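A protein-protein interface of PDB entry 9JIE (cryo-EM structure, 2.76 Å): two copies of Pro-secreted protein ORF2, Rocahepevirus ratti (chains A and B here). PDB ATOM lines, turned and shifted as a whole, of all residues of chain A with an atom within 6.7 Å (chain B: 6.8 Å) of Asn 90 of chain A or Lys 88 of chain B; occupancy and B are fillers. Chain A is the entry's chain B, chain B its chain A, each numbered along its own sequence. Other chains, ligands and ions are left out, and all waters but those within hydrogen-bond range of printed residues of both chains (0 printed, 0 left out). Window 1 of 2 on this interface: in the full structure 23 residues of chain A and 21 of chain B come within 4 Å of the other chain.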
ATOM      1  N   VAL A  17     -14.193   2.136  14.386  1.00  0.00           N
ATOM      2  CA  VAL A  17     -14.895   2.023  15.657  1.00  0.00           C
ATOM      3  C   VAL A  17     -15.100   3.414  16.244  1.00  0.00           C
ATOM      4  O   VAL A  17     -14.156   4.208  16.321  1.00  0.00           O
ATOM      5  CB  VAL A  17     -14.140   1.099  16.632  1.00  0.00           C
ATOM      6  CG1 VAL A  17     -14.080  -0.313  16.108  1.00  0.00           C
ATOM      7  CG2 VAL A  17     -12.745   1.596  16.829  1.00  0.00           C
ATOM      8  N   LEU A  85      -6.869  -8.351  15.352  1.00  0.00           N
ATOM      9  CA  LEU A  85      -6.372  -7.333  14.442  1.00  0.00           C
ATOM     10  C   LEU A  85      -4.900  -7.579  14.149  1.00  0.00           C
ATOM     11  O   LEU A  85      -4.161  -8.092  14.993  1.00  0.00           O
ATOM     12  CB  LEU A  85      -6.560  -5.918  15.012  1.00  0.00           C
ATOM     13  CG  LEU A  85      -7.964  -5.506  15.457  1.00  0.00           C
ATOM     14  CD1 LEU A  85      -7.906  -4.216  16.249  1.00  0.00           C
ATOM     15  CD2 LEU A  85      -8.887  -5.357  14.263  1.00  0.00           C
ATOM     16  N   LYS A  88      -1.563  -2.981  16.158  1.00  0.00           N
ATOM     17  CA  LYS A  88      -2.237  -2.336  17.272  1.00  0.00           C
ATOM     18  C   LYS A  88      -3.474  -1.583  16.797  1.00  0.00           C
ATOM     19  O   LYS A  88      -3.523  -1.069  15.676  1.00  0.00           O
ATOM     20  CB  LYS A  88      -1.283  -1.374  17.978  1.00  0.00           C
ATOM     21  CG  LYS A  88      -0.119  -2.063  18.652  1.00  0.00           C
ATOM     22  CD  LYS A  88       1.085  -1.149  18.716  1.00  0.00           C
ATOM     23  CE  LYS A  88       2.326  -1.912  19.136  1.00  0.00           C
ATOM     24  NZ  LYS A  88       1.981  -3.210  19.777  1.00  0.00           N
ATOM     25  N   ILE A  89      -4.483  -1.527  17.660  1.00  0.00           N
ATOM     26  CA  ILE A  89      -5.683  -0.748  17.374  1.00  0.00           C
ATOM     27  C   ILE A  89      -5.372   0.724  17.618  1.00  0.00           C
ATOM     28  O   ILE A  89      -4.933   1.110  18.706  1.00  0.00           O
ATOM     29  CB  ILE A  89      -6.875  -1.223  18.223  1.00  0.00           C
ATOM     30  CG1 ILE A  89      -8.100  -0.331  17.992  1.00  0.00           C
ATOM     31  CG2 ILE A  89      -6.515  -1.308  19.701  1.00  0.00           C
ATOM     32  CD1 ILE A  89      -8.939  -0.730  16.799  1.00  0.00           C
ATOM     33  N   ASN A  90      -5.572   1.547  16.593  1.00  0.00           N
ATOM     34  CA  ASN A  90      -5.275   2.971  16.662  1.00  0.00           C
ATOM     35  C   ASN A  90      -6.558   3.727  16.978  1.00  0.00           C
ATOM     36  O   ASN A  90      -7.532   3.642  16.225  1.00  0.00           O
ATOM     37  CB  ASN A  90      -4.665   3.464  15.351  1.00  0.00           C
ATOM     38  CG  ASN A  90      -4.349   4.946  15.377  1.00  0.00           C
ATOM     39  OD1 ASN A  90      -3.872   5.472  16.382  1.00  0.00           O
ATOM     40  ND2 ASN A  90      -4.613   5.626  14.269  1.00  0.00           N
ATOM     41  N   PHE A  91      -6.552   4.466  18.085  1.00  0.00           N
ATOM     42  CA  PHE A  91      -7.718   5.208  18.539  1.00  0.00           C
ATOM     43  C   PHE A  91      -7.309   6.611  18.961  1.00  0.00           C
ATOM     44  O   PHE A  91      -6.169   6.848  19.373  1.00  0.00           O
ATOM     45  CB  PHE A  91      -8.430   4.492  19.699  1.00  0.00           C
ATOM     46  CG  PHE A  91      -7.631   4.446  20.971  1.00  0.00           C
ATOM     47  CD1 PHE A  91      -6.544   3.601  21.093  1.00  0.00           C
ATOM     48  CD2 PHE A  91      -7.975   5.242  22.047  1.00  0.00           C
ATOM     49  CE1 PHE A  91      -5.812   3.558  22.259  1.00  0.00           C
ATOM     50  CE2 PHE A  91      -7.245   5.201  23.215  1.00  0.00           C
ATOM     51  CZ  PHE A  91      -6.164   4.357  23.320  1.00  0.00           C
ATOM     52  N   TRP A  92      -8.256   7.541  18.855  1.00  0.00           N
ATOM     53  CA  TRP A  92      -7.996   8.941  19.149  1.00  0.00           C
ATOM     54  C   TRP A  92      -9.291   9.608  19.584  1.00  0.00           C
ATOM     55  O   TRP A  92     -10.387   9.090  19.354  1.00  0.00           O
ATOM     56  CB  TRP A  92      -7.403   9.669  17.935  1.00  0.00           C
ATOM     57  CG  TRP A  92      -8.299   9.661  16.737  1.00  0.00           C
ATOM     58  CD1 TRP A  92      -9.189  10.627  16.375  1.00  0.00           C
ATOM     59  CD2 TRP A  92      -8.395   8.636  15.741  1.00  0.00           C
ATOM     60  NE1 TRP A  92      -9.833  10.270  15.217  1.00  0.00           N
ATOM     61  CE2 TRP A  92      -9.362   9.051  14.806  1.00  0.00           C
ATOM     62  CE3 TRP A  92      -7.755   7.408  15.549  1.00  0.00           C
ATOM     63  CZ2 TRP A  92      -9.705   8.283  13.698  1.00  0.00           C
ATOM     64  CZ3 TRP A  92      -8.098   6.648  14.448  1.00  0.00           C
ATOM     65  CH2 TRP A  92      -9.064   7.087  13.537  1.00  0.00           C
ATOM     66  N   ALA A  99      -4.469  11.882  20.396  1.00  0.00           N
ATOM     67  CA  ALA A  99      -4.488  10.473  20.038  1.00  0.00           C
ATOM     68  C   ALA A  99      -4.242   9.607  21.265  1.00  0.00           C
ATOM     69  O   ALA A  99      -3.625  10.034  22.245  1.00  0.00           O
ATOM     70  CB  ALA A  99      -3.437  10.160  18.966  1.00  0.00           C
ATOM     71  N   GLY A 100      -4.738   8.376  21.198  1.00  0.00           N
ATOM     72  CA  GLY A 100      -4.564   7.412  22.264  1.00  0.00           C
ATOM     73  C   GLY A 100      -3.602   6.304  21.879  1.00  0.00           C
ATOM     74  O   GLY A 100      -3.472   5.951  20.710  1.00  0.00           O
ATOM     75  N   TYR A 101      -2.914   5.754  22.886  1.00  0.00           N
ATOM     76  CA  TYR A 101      -1.982   4.650  22.706  1.00  0.00           C
ATOM     77  C   TYR A 101      -2.400   3.497  23.605  1.00  0.00           C
ATOM     78  O   TYR A 101      -2.782   3.712  24.760  1.00  0.00           O
ATOM     79  CB  TYR A 101      -0.546   5.079  23.010  1.00  0.00           C
ATOM     80  CG  TYR A 101      -0.393   5.873  24.283  1.00  0.00           C
ATOM     81  CD1 TYR A 101      -0.527   5.265  25.521  1.00  0.00           C
ATOM     82  CD2 TYR A 101      -0.110   7.230  24.247  1.00  0.00           C
ATOM     83  CE1 TYR A 101      -0.384   5.987  26.689  1.00  0.00           C
ATOM     84  CE2 TYR A 101       0.030   7.960  25.408  1.00  0.00           C
ATOM     85  CZ  TYR A 101      -0.107   7.334  26.626  1.00  0.00           C
ATOM     86  OH  TYR A 101       0.036   8.059  27.787  1.00  0.00           O
ATOM     87  N   THR A 102      -2.339   2.285  23.071  1.00  0.00           N
ATOM     88  CA  THR A 102      -2.846   1.111  23.761  1.00  0.00           C
ATOM     89  C   THR A 102      -1.884   0.679  24.864  1.00  0.00           C
ATOM     90  O   THR A 102      -0.824   1.273  25.073  1.00  0.00           O
ATOM     91  CB  THR A 102      -3.080  -0.021  22.767  1.00  0.00           C
ATOM     92  OG1 THR A 102      -1.863  -0.303  22.068  1.00  0.00           O
ATOM     93  CG2 THR A 102      -4.133   0.394  21.762  1.00  0.00           C
ATOM     94  N   ASP A 111      -3.216  -6.144  18.692  1.00  0.00           N
ATOM     95  CA  ASP A 111      -4.354  -5.834  19.540  1.00  0.00           C
ATOM     96  C   ASP A 111      -5.616  -6.485  18.992  1.00  0.00           C
ATOM     97  O   ASP A 111      -5.635  -7.046  17.894  1.00  0.00           O
ATOM     98  CB  ASP A 111      -4.535  -4.319  19.657  1.00  0.00           C
ATOM     99  CG  ASP A 111      -3.366  -3.650  20.345  1.00  0.00           C
ATOM    100  OD1 ASP A 111      -2.346  -4.328  20.587  1.00  0.00           O
ATOM    101  OD2 ASP A 111      -3.469  -2.447  20.649  1.00  0.00           O
ATOM    102  N   MET A 133      -5.047   9.054  28.905  1.00  0.00           N
ATOM    103  CA  MET A 133      -4.439  10.085  28.072  1.00  0.00           C
ATOM    104  C   MET A 133      -5.467  10.880  27.271  1.00  0.00           C
ATOM    105  O   MET A 133      -5.171  12.004  26.853  1.00  0.00           O
ATOM    106  CB  MET A 133      -3.410   9.446  27.137  1.00  0.00           C
ATOM    107  CG  MET A 133      -4.003   8.785  25.904  1.00  0.00           C
ATOM    108  SD  MET A 133      -3.083   7.315  25.410  1.00  0.00           S
ATOM    109  CE  MET A 133      -3.898   6.057  26.387  1.00  0.00           C
ATOM    110  N   THR A 142     -12.652   7.794  18.804  1.00  0.00           N
ATOM    111  CA  THR A 142     -12.747   7.149  17.502  1.00  0.00           C
ATOM    112  C   THR A 142     -11.484   6.333  17.261  1.00  0.00           C
ATOM    113  O   THR A 142     -10.377   6.787  17.566  1.00  0.00           O
ATOM    114  CB  THR A 142     -12.934   8.188  16.392  1.00  0.00           C
ATOM    115  OG1 THR A 142     -14.213   8.818  16.539  1.00  0.00           O
ATOM    116  CG2 THR A 142     -12.862   7.539  15.028  1.00  0.00           C
ATOM    117  N   GLY A 143     -11.650   5.122  16.718  1.00  0.00           N
ATOM    118  CA  GLY A 143     -10.541   4.215  16.530  1.00  0.00           C
ATOM    119  C   GLY A 143     -10.547   3.586  15.147  1.00  0.00           C
ATOM    120  O   GLY A 143     -11.460   3.799  14.344  1.00  0.00           O
ATOM    121  N   LEU A 144      -9.505   2.796  14.888  1.00  0.00           N
ATOM    122  CA  LEU A 144      -9.310   2.181  13.582  1.00  0.00           C
ATOM    123  C   LEU A 144      -8.388   0.977  13.725  1.00  0.00           C
ATOM    124  O   LEU A 144      -7.432   1.012  14.504  1.00  0.00           O
ATOM    125  CB  LEU A 144      -8.720   3.188  12.588  1.00  0.00           C
ATOM    126  CG  LEU A 144      -8.497   2.724  11.149  1.00  0.00           C
ATOM    127  CD1 LEU A 144      -9.798   2.779  10.376  1.00  0.00           C
ATOM    128  CD2 LEU A 144      -7.435   3.574  10.481  1.00  0.00           C
ATOM    129  N   GLY A 145      -8.673  -0.078  12.962  1.00  0.00           N
ATOM    130  CA  GLY A 145      -7.851  -1.276  12.989  1.00  0.00           C
ATOM    131  C   GLY A 145      -8.065  -2.121  11.753  1.00  0.00           C
ATOM    132  O   GLY A 145      -8.972  -1.881  10.954  1.00  0.00           O
ATOM    133  N   LEU B  85      -2.379  12.415   9.635  1.00  0.00           N
ATOM    134  CA  LEU B  85      -3.286  11.377  10.094  1.00  0.00           C
ATOM    135  C   LEU B  85      -3.842  11.750  11.460  1.00  0.00           C
ATOM    136  O   LEU B  85      -3.212  12.487  12.221  1.00  0.00           O
ATOM    137  CB  LEU B  85      -2.587  10.009  10.172  1.00  0.00           C
ATOM    138  CG  LEU B  85      -1.864   9.497   8.923  1.00  0.00           C
ATOM    139  CD1 LEU B  85      -0.978   8.319   9.272  1.00  0.00           C
ATOM    140  CD2 LEU B  85      -2.856   9.115   7.842  1.00  0.00           C
ATOM    141  N   MET B  86      -5.038  11.240  11.759  1.00  0.00           N
ATOM    142  CA  MET B  86      -5.618  11.336  13.099  1.00  0.00           C
ATOM    143  C   MET B  86      -5.188  10.100  13.873  1.00  0.00           C
ATOM    144  O   MET B  86      -5.677   8.996  13.626  1.00  0.00           O
ATOM    145  CB  MET B  86      -7.137  11.449  13.045  1.00  0.00           C
ATOM    146  CG  MET B  86      -7.660  12.860  12.895  1.00  0.00           C
ATOM    147  SD  MET B  86      -9.453  12.958  13.035  1.00  0.00           S
ATOM    148  CE  MET B  86      -9.956  12.093  11.556  1.00  0.00           C
ATOM    149  N   GLY B  87      -4.276  10.281  14.812  1.00  0.00           N
ATOM    150  CA  GLY B  87      -3.722   9.169  15.550  1.00  0.00           C
ATOM    151  C   GLY B  87      -2.405   8.704  14.968  1.00  0.00           C
ATOM    152  O   GLY B  87      -1.816   9.322  14.077  1.00  0.00           O
ATOM    153  N   LYS B  88      -1.940   7.578  15.496  1.00  0.00           N
ATOM    154  CA  LYS B  88      -0.671   7.012  15.069  1.00  0.00           C
ATOM    155  C   LYS B  88      -0.861   6.111  13.855  1.00  0.00           C
ATOM    156  O   LYS B  88      -1.900   5.466  13.690  1.00  0.00           O
ATOM    157  CB  LYS B  88      -0.035   6.225  16.213  1.00  0.00           C
ATOM    158  CG  LYS B  88       0.364   7.086  17.389  1.00  0.00           C
ATOM    159  CD  LYS B  88       0.331   6.296  18.676  1.00  0.00           C
ATOM    160  CE  LYS B  88       0.452   7.213  19.876  1.00  0.00           C
ATOM    161  NZ  LYS B  88       0.978   8.551  19.489  1.00  0.00           N
ATOM    162  N   ILE B  89       0.155   6.074  12.999  1.00  0.00           N
ATOM    163  CA  ILE B  89       0.138   5.185  11.844  1.00  0.00           C
ATOM    164  C   ILE B  89       0.448   3.771  12.320  1.00  0.00           C
ATOM    165  O   ILE B  89       1.478   3.526  12.955  1.00  0.00           O
ATOM    166  CB  ILE B  89       1.129   5.651  10.764  1.00  0.00           C
ATOM    167  CG1 ILE B  89       0.997   4.800   9.498  1.00  0.00           C
ATOM    168  CG2 ILE B  89       2.560   5.667  11.285  1.00  0.00           C
ATOM    169  CD1 ILE B  89       1.703   5.378   8.293  1.00  0.00           C
ATOM    170  N   ASN B  90      -0.455   2.837  12.032  1.00  0.00           N
ATOM    171  CA  ASN B  90      -0.326   1.456  12.477  1.00  0.00           C
ATOM    172  C   ASN B  90       0.281   0.631  11.349  1.00  0.00           C
ATOM    173  O   ASN B  90      -0.308   0.522  10.270  1.00  0.00           O
ATOM    174  CB  ASN B  90      -1.683   0.890  12.894  1.00  0.00           C
ATOM    175  CG  ASN B  90      -1.590  -0.542  13.380  1.00  0.00           C
ATOM    176  OD1 ASN B  90      -0.657  -0.909  14.093  1.00  0.00           O
ATOM    177  ND2 ASN B  90      -2.563  -1.361  12.998  1.00  0.00           N
ATOM    178  N   PHE B  91       1.451   0.051  11.606  1.00  0.00           N
ATOM    179  CA  PHE B  91       2.177  -0.724  10.611  1.00  0.00           C
ATOM    180  C   PHE B  91       2.644  -2.037  11.222  1.00  0.00           C
ATOM    181  O   PHE B  91       2.922  -2.121  12.422  1.00  0.00           O
ATOM    182  CB  PHE B  91       3.379   0.054  10.052  1.00  0.00           C
ATOM    183  CG  PHE B  91       4.464   0.307  11.058  1.00  0.00           C
ATOM    184  CD1 PHE B  91       4.299   1.252  12.054  1.00  0.00           C
ATOM    185  CD2 PHE B  91       5.652  -0.396  11.003  1.00  0.00           C
ATOM    186  CE1 PHE B  91       5.294   1.485  12.978  1.00  0.00           C
ATOM    187  CE2 PHE B  91       6.651  -0.166  11.925  1.00  0.00           C
ATOM    188  CZ  PHE B  91       6.472   0.775  12.913  1.00  0.00           C
ATOM    189  N   THR B 102       5.417   3.074  16.366  1.00  0.00           N
ATOM    190  CA  THR B 102       6.057   4.274  15.849  1.00  0.00           C
ATOM    191  C   THR B 102       6.951   4.911  16.909  1.00  0.00           C
ATOM    192  O   THR B 102       7.094   4.412  18.028  1.00  0.00           O
ATOM    193  CB  THR B 102       5.005   5.266  15.364  1.00  0.00           C
ATOM    194  OG1 THR B 102       4.100   5.566  16.432  1.00  0.00           O
ATOM    195  CG2 THR B 102       4.226   4.669  14.214  1.00  0.00           C
ATOM    196  N   ASN B 104       6.609   8.064  18.281  1.00  0.00           N
ATOM    197  CA  ASN B 104       5.811   8.763  19.288  1.00  0.00           C
ATOM    198  C   ASN B 104       4.690   7.860  19.804  1.00  0.00           C
ATOM    199  O   ASN B 104       3.504   8.179  19.744  1.00  0.00           O
ATOM    200  CB  ASN B 104       5.260  10.065  18.717  1.00  0.00           C
ATOM    201  CG  ASN B 104       6.348  11.074  18.412  1.00  0.00           C
ATOM    202  OD1 ASN B 104       7.324  11.194  19.152  1.00  0.00           O
ATOM    203  ND2 ASN B 104       6.185  11.808  17.318  1.00  0.00           N
ATOM    204  N   TYR B 105       5.101   6.702  20.322  1.00  0.00           N
ATOM    205  CA  TYR B 105       4.173   5.732  20.886  1.00  0.00           C
ATOM    206  C   TYR B 105       3.689   6.107  22.281  1.00  0.00           C
ATOM    207  O   TYR B 105       2.661   5.582  22.723  1.00  0.00           O
ATOM    208  CB  TYR B 105       4.828   4.351  20.922  1.00  0.00           C
ATOM    209  CG  TYR B 105       6.126   4.305  21.699  1.00  0.00           C
ATOM    210  CD1 TYR B 105       6.134   4.080  23.065  1.00  0.00           C
ATOM    211  CD2 TYR B 105       7.345   4.488  21.065  1.00  0.00           C
ATOM    212  CE1 TYR B 105       7.311   4.040  23.776  1.00  0.00           C
ATOM    213  CE2 TYR B 105       8.528   4.447  21.768  1.00  0.00           C
ATOM    214  CZ  TYR B 105       8.505   4.221  23.123  1.00  0.00           C
ATOM    215  OH  TYR B 105       9.682   4.179  23.831  1.00  0.00           O
ATOM    216  N   ASN B 106       4.401   6.991  22.985  1.00  0.00           N
ATOM    217  CA  ASN B 106       4.039   7.387  24.338  1.00  0.00           C
ATOM    218  C   ASN B 106       3.211   8.659  24.408  1.00  0.00           C
ATOM    219  O   ASN B 106       2.619   8.930  25.457  1.00  0.00           O
ATOM    220  CB  ASN B 106       5.301   7.588  25.190  1.00  0.00           C
ATOM    221  CG  ASN B 106       5.749   6.319  25.871  1.00  0.00           C
ATOM    222  OD1 ASN B 106       4.937   5.451  26.181  1.00  0.00           O
ATOM    223  ND2 ASN B 106       7.048   6.205  26.117  1.00  0.00           N
ATOM    224  N   THR B 107       3.164   9.444  23.340  1.00  0.00           N
ATOM    225  CA  THR B 107       2.501  10.737  23.351  1.00  0.00           C
ATOM    226  C   THR B 107       1.160  10.665  22.632  1.00  0.00           C
ATOM    227  O   THR B 107       0.830   9.685  21.962  1.00  0.00           O
ATOM    228  CB  THR B 107       3.392  11.801  22.704  1.00  0.00           C
ATOM    229  OG1 THR B 107       3.688  11.420  21.357  1.00  0.00           O
ATOM    230  CG2 THR B 107       4.691  11.950  23.481  1.00  0.00           C
ATOM    231  N   THR B 108       0.382  11.732  22.783  1.00  0.00           N
ATOM    232  CA  THR B 108      -0.892  11.873  22.096  1.00  0.00           C
ATOM    233  C   THR B 108      -0.750  12.557  20.746  1.00  0.00           C
ATOM    234  O   THR B 108      -1.762  12.793  20.078  1.00  0.00           O
ATOM    235  CB  THR B 108      -1.881  12.657  22.963  1.00  0.00           C
ATOM    236  OG1 THR B 108      -1.339  13.951  23.254  1.00  0.00           O
ATOM    237  CG2 THR B 108      -2.152  11.922  24.266  1.00  0.00           C
ATOM    238  N   ASP B 109       0.472  12.889  20.339  1.00  0.00           N
ATOM    239  CA  ASP B 109       0.694  13.508  19.041  1.00  0.00           C
ATOM    240  C   ASP B 109       0.430  12.502  17.929  1.00  0.00           C
ATOM    241  O   ASP B 109       0.834  11.338  18.019  1.00  0.00           O
ATOM    242  CB  ASP B 109       2.121  14.043  18.945  1.00  0.00           C
ATOM    243  CG  ASP B 109       2.344  15.264  19.816  1.00  0.00           C
ATOM    244  OD1 ASP B 109       1.347  15.863  20.269  1.00  0.00           O
ATOM    245  OD2 ASP B 109       3.518  15.623  20.048  1.00  0.00           O
ATOM    246  N   SER B 110      -0.247  12.952  16.881  1.00  0.00           N
ATOM    247  CA  SER B 110      -0.578  12.083  15.769  1.00  0.00           C
ATOM    248  C   SER B 110       0.619  11.924  14.836  1.00  0.00           C
ATOM    249  O   SER B 110       1.618  12.642  14.932  1.00  0.00           O
ATOM    250  CB  SER B 110      -1.778  12.632  15.001  1.00  0.00           C
ATOM    251  OG  SER B 110      -2.805  13.038  15.889  1.00  0.00           O
ATOM    252  N   ASP B 111       0.505  10.964  13.925  1.00  0.00           N
ATOM    253  CA  ASP B 111       1.564  10.636  12.983  1.00  0.00           C
ATOM    254  C   ASP B 111       1.191  11.105  11.583  1.00  0.00           C
ATOM    255  O   ASP B 111       0.083  11.583  11.331  1.00  0.00           O
ATOM    256  CB  ASP B 111       1.846   9.131  12.988  1.00  0.00           C
ATOM    257  CG  ASP B 111       2.323   8.633  14.337  1.00  0.00           C
ATOM    258  OD1 ASP B 111       2.298   9.419  15.307  1.00  0.00           O
ATOM    259  OD2 ASP B 111       2.719   7.455  14.429  1.00  0.00           O
ATOM    260  N   SER B 112       2.143  10.953  10.666  1.00  0.00           N
ATOM    261  CA  SER B 112       1.986  11.453   9.309  1.00  0.00           C
ATOM    262  C   SER B 112       2.720  10.543   8.339  1.00  0.00           C
ATOM    263  O   SER B 112       3.616   9.786   8.720  1.00  0.00           O
ATOM    264  CB  SER B 112       2.506  12.887   9.179  1.00  0.00           C
ATOM    265  OG  SER B 112       3.897  12.943   9.420  1.00  0.00           O
ATOM    266  N   LEU B 144      -1.306   1.121   8.058  1.00  0.00           N
ATOM    267  CA  LEU B 144      -2.689   1.574   8.022  1.00  0.00           C
ATOM    268  C   LEU B 144      -2.827   2.846   8.850  1.00  0.00           C
ATOM    269  O   LEU B 144      -2.214   2.968   9.912  1.00  0.00           O
ATOM    270  CB  LEU B 144      -3.635   0.492   8.556  1.00  0.00           C
ATOM    271  CG  LEU B 144      -5.133   0.800   8.560  1.00  0.00           C
ATOM    272  CD1 LEU B 144      -5.734   0.494   7.203  1.00  0.00           C
ATOM    273  CD2 LEU B 144      -5.833   0.013   9.652  1.00  0.00           C
ATOM    274  N   GLY B 145      -3.642   3.781   8.361  1.00  0.00           N
ATOM    275  CA  GLY B 145      -3.880   5.028   9.068  1.00  0.00           C
ATOM    276  C   GLY B 145      -5.136   5.709   8.574  1.00  0.00           C
ATOM    277  O   GLY B 145      -5.755   5.290   7.594  1.00  0.00           O
ATOM    278  N   ALA B 146      -5.508   6.779   9.275  1.00  0.00           N
ATOM    279  CA  ALA B 146      -6.690   7.569   8.944  1.00  0.00           C
ATOM    280  C   ALA B 146      -6.298   9.033   8.808  1.00  0.00           C
ATOM    281  O   ALA B 146      -5.730   9.611   9.738  1.00  0.00           O
ATOM    282  CB  ALA B 146      -7.779   7.410  10.008  1.00  0.00           C
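SD of Met 86 of chain B lies within hydrogen-bond range of NE1 of Trp 92 of chain A, 3.5 Å away. The side-chain amide nitrogen (ND2) of Asn 90 of chain A lies within hydrogen-bond range of the backbone carbonyl oxygen (O) of Lys 88 of chain B (2.8 Å). O of Lys 88 of chain A is in hydrogen-bond range of ND2 of Asn 90 of chain B. The backbone NH (N) of Ala 99 of chain A sits at hydrogen-bond distance from the backbone carbonyl oxygen (O) of Thr 108 of chain B, at 2.9 Å.
The backbone carbonyl oxygen of Ala 146 of chain B is in hydrogen-bond range of the backbone NH of Met 86 of chain B (2.7 Å). The backbone NH of Asp 111 of chain B lies within hydrogen-bond range of the backbone carbonyl oxygen of Gly 87 of chain B, 2.8 Å away. The side-chain amino group (NZ) of Lys 88 of chain B sits at hydrogen-bond distance from the backbone carbonyl oxygen (O) of Asn 104 of chain B. The backbone carbonyl oxygen (O) of Thr 107 of chain B sits at hydrogen-bond distance from the side-chain amino group (NZ) of Lys 88 of chain B, 2.7 Å away. The backbone NH (N) of Leu 144 of chain B is in hydrogen-bond range of the backbone carbonyl oxygen (O) of Asn 90 of chain B (2.5 Å). The backbone NH of Tyr 101 of chain A sits at hydrogen-bond distance from the side-chain sulfur of Met 133 of chain A (3.0 Å).
Among the printed residues, merely in contact across the chains: Asn 90 of chain A with Met 86 of chain B (3.6 Å), Asn 90 of chain A with Gly 87 of chain B (3.8 Å), Trp 92 of chain A with Ala 146 of chain B (3.8 Å), Ala 99 of chain A with Gly 87 of chain B (3.6 Å), Tyr 101 of chain A with Lys 88 of chain B (3.9 Å), Tyr 101 of chain A with Tyr 105 of chain B (3.3 Å), Tyr 101 of chain A with Asn 106 of chain B (2.8 Å), Tyr 101 of chain A with Thr 107 of chain B (3.5 Å), Met 133 of chain A with Thr 108 of chain B (3.98 Å), Leu 144 of chain A with Leu 144 of chain B (3.99 Å), Leu 144 of chain A with Gly 145 of chain B (3.7 Å), Leu 144 of chain A with Ala 146 of chain B (3.9 Å) and Gly 145 of chain A with Leu 144 of chain B (3.7 Å).
Of the printed residues of chain B, Asn 90 of chain A touches Met 86 (3.6 Å), Gly 87 (3.8 Å) and Lys 88 (2.8 Å). Of the printed residues of chain A, Lys 88 of chain B touches Asn 90 and Tyr 101. Of the printed residues of chain B, Ala 99 of chain A touches Gly 87 and Thr 108. Printed residues of chain A within 4 Å of Gly 87 of chain B: Asn 90 and Ala 99. Of the printed residues of chain B, Leu 144 of chain A touches Leu 144 (3.99 Å), Gly 145 (3.7 Å) and Ala 146 (3.9 Å). The nearest residue of chain B that does not touch Asn 90 of chain A is Asn 90 of chain B (4.6 Å). The nearest residue of chain A that does not touch Lys 88 of chain B is Gly 100 of chain A (4.2 Å).
Printed residues of chain A that touch a printed residue of chain B: Lys 88, Asn 90, Trp 92, Ala 99, Tyr 101, Met 133, Leu 144 and Gly 145. Hydrophobic or aromatic side chains of chain A within 4 Å of the printed part of chain B: Trp 92, Ala 99, Tyr 101, Met 133 and Leu 144. Of the 20 printed residues of chain B, 11 touch a printed residue of chain A. Printed residues of chain B that touch a printed residue of chain A: Met 86, Gly 87, Lys 88, Asn 90, Tyr 105, Asn 106, Thr 107, Thr 108, Leu 144, Gly 145 and Ala 146. Among the printed residues, 17 pairs touch across the chains.
Lys 88 of chain A touches Asn 90 of chain B, and with the chains exchanged Asn 90 of chain A touches Lys 88 of chain B. Leu 144 of chain B touches its own counterpart, Leu 144 of chain A. Leu 144 of chain A touches Gly 145 of chain B, and with the chains exchanged Gly 145 of chain A touches Leu 144 of chain B. Positions printed for both chains: 85, 88, 89, 90, 91, 102, 111, 144 and 145. Of the 17 pairs that touch across the chains among the printed residues, 5 have their exchanged pair printed and touching as well.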
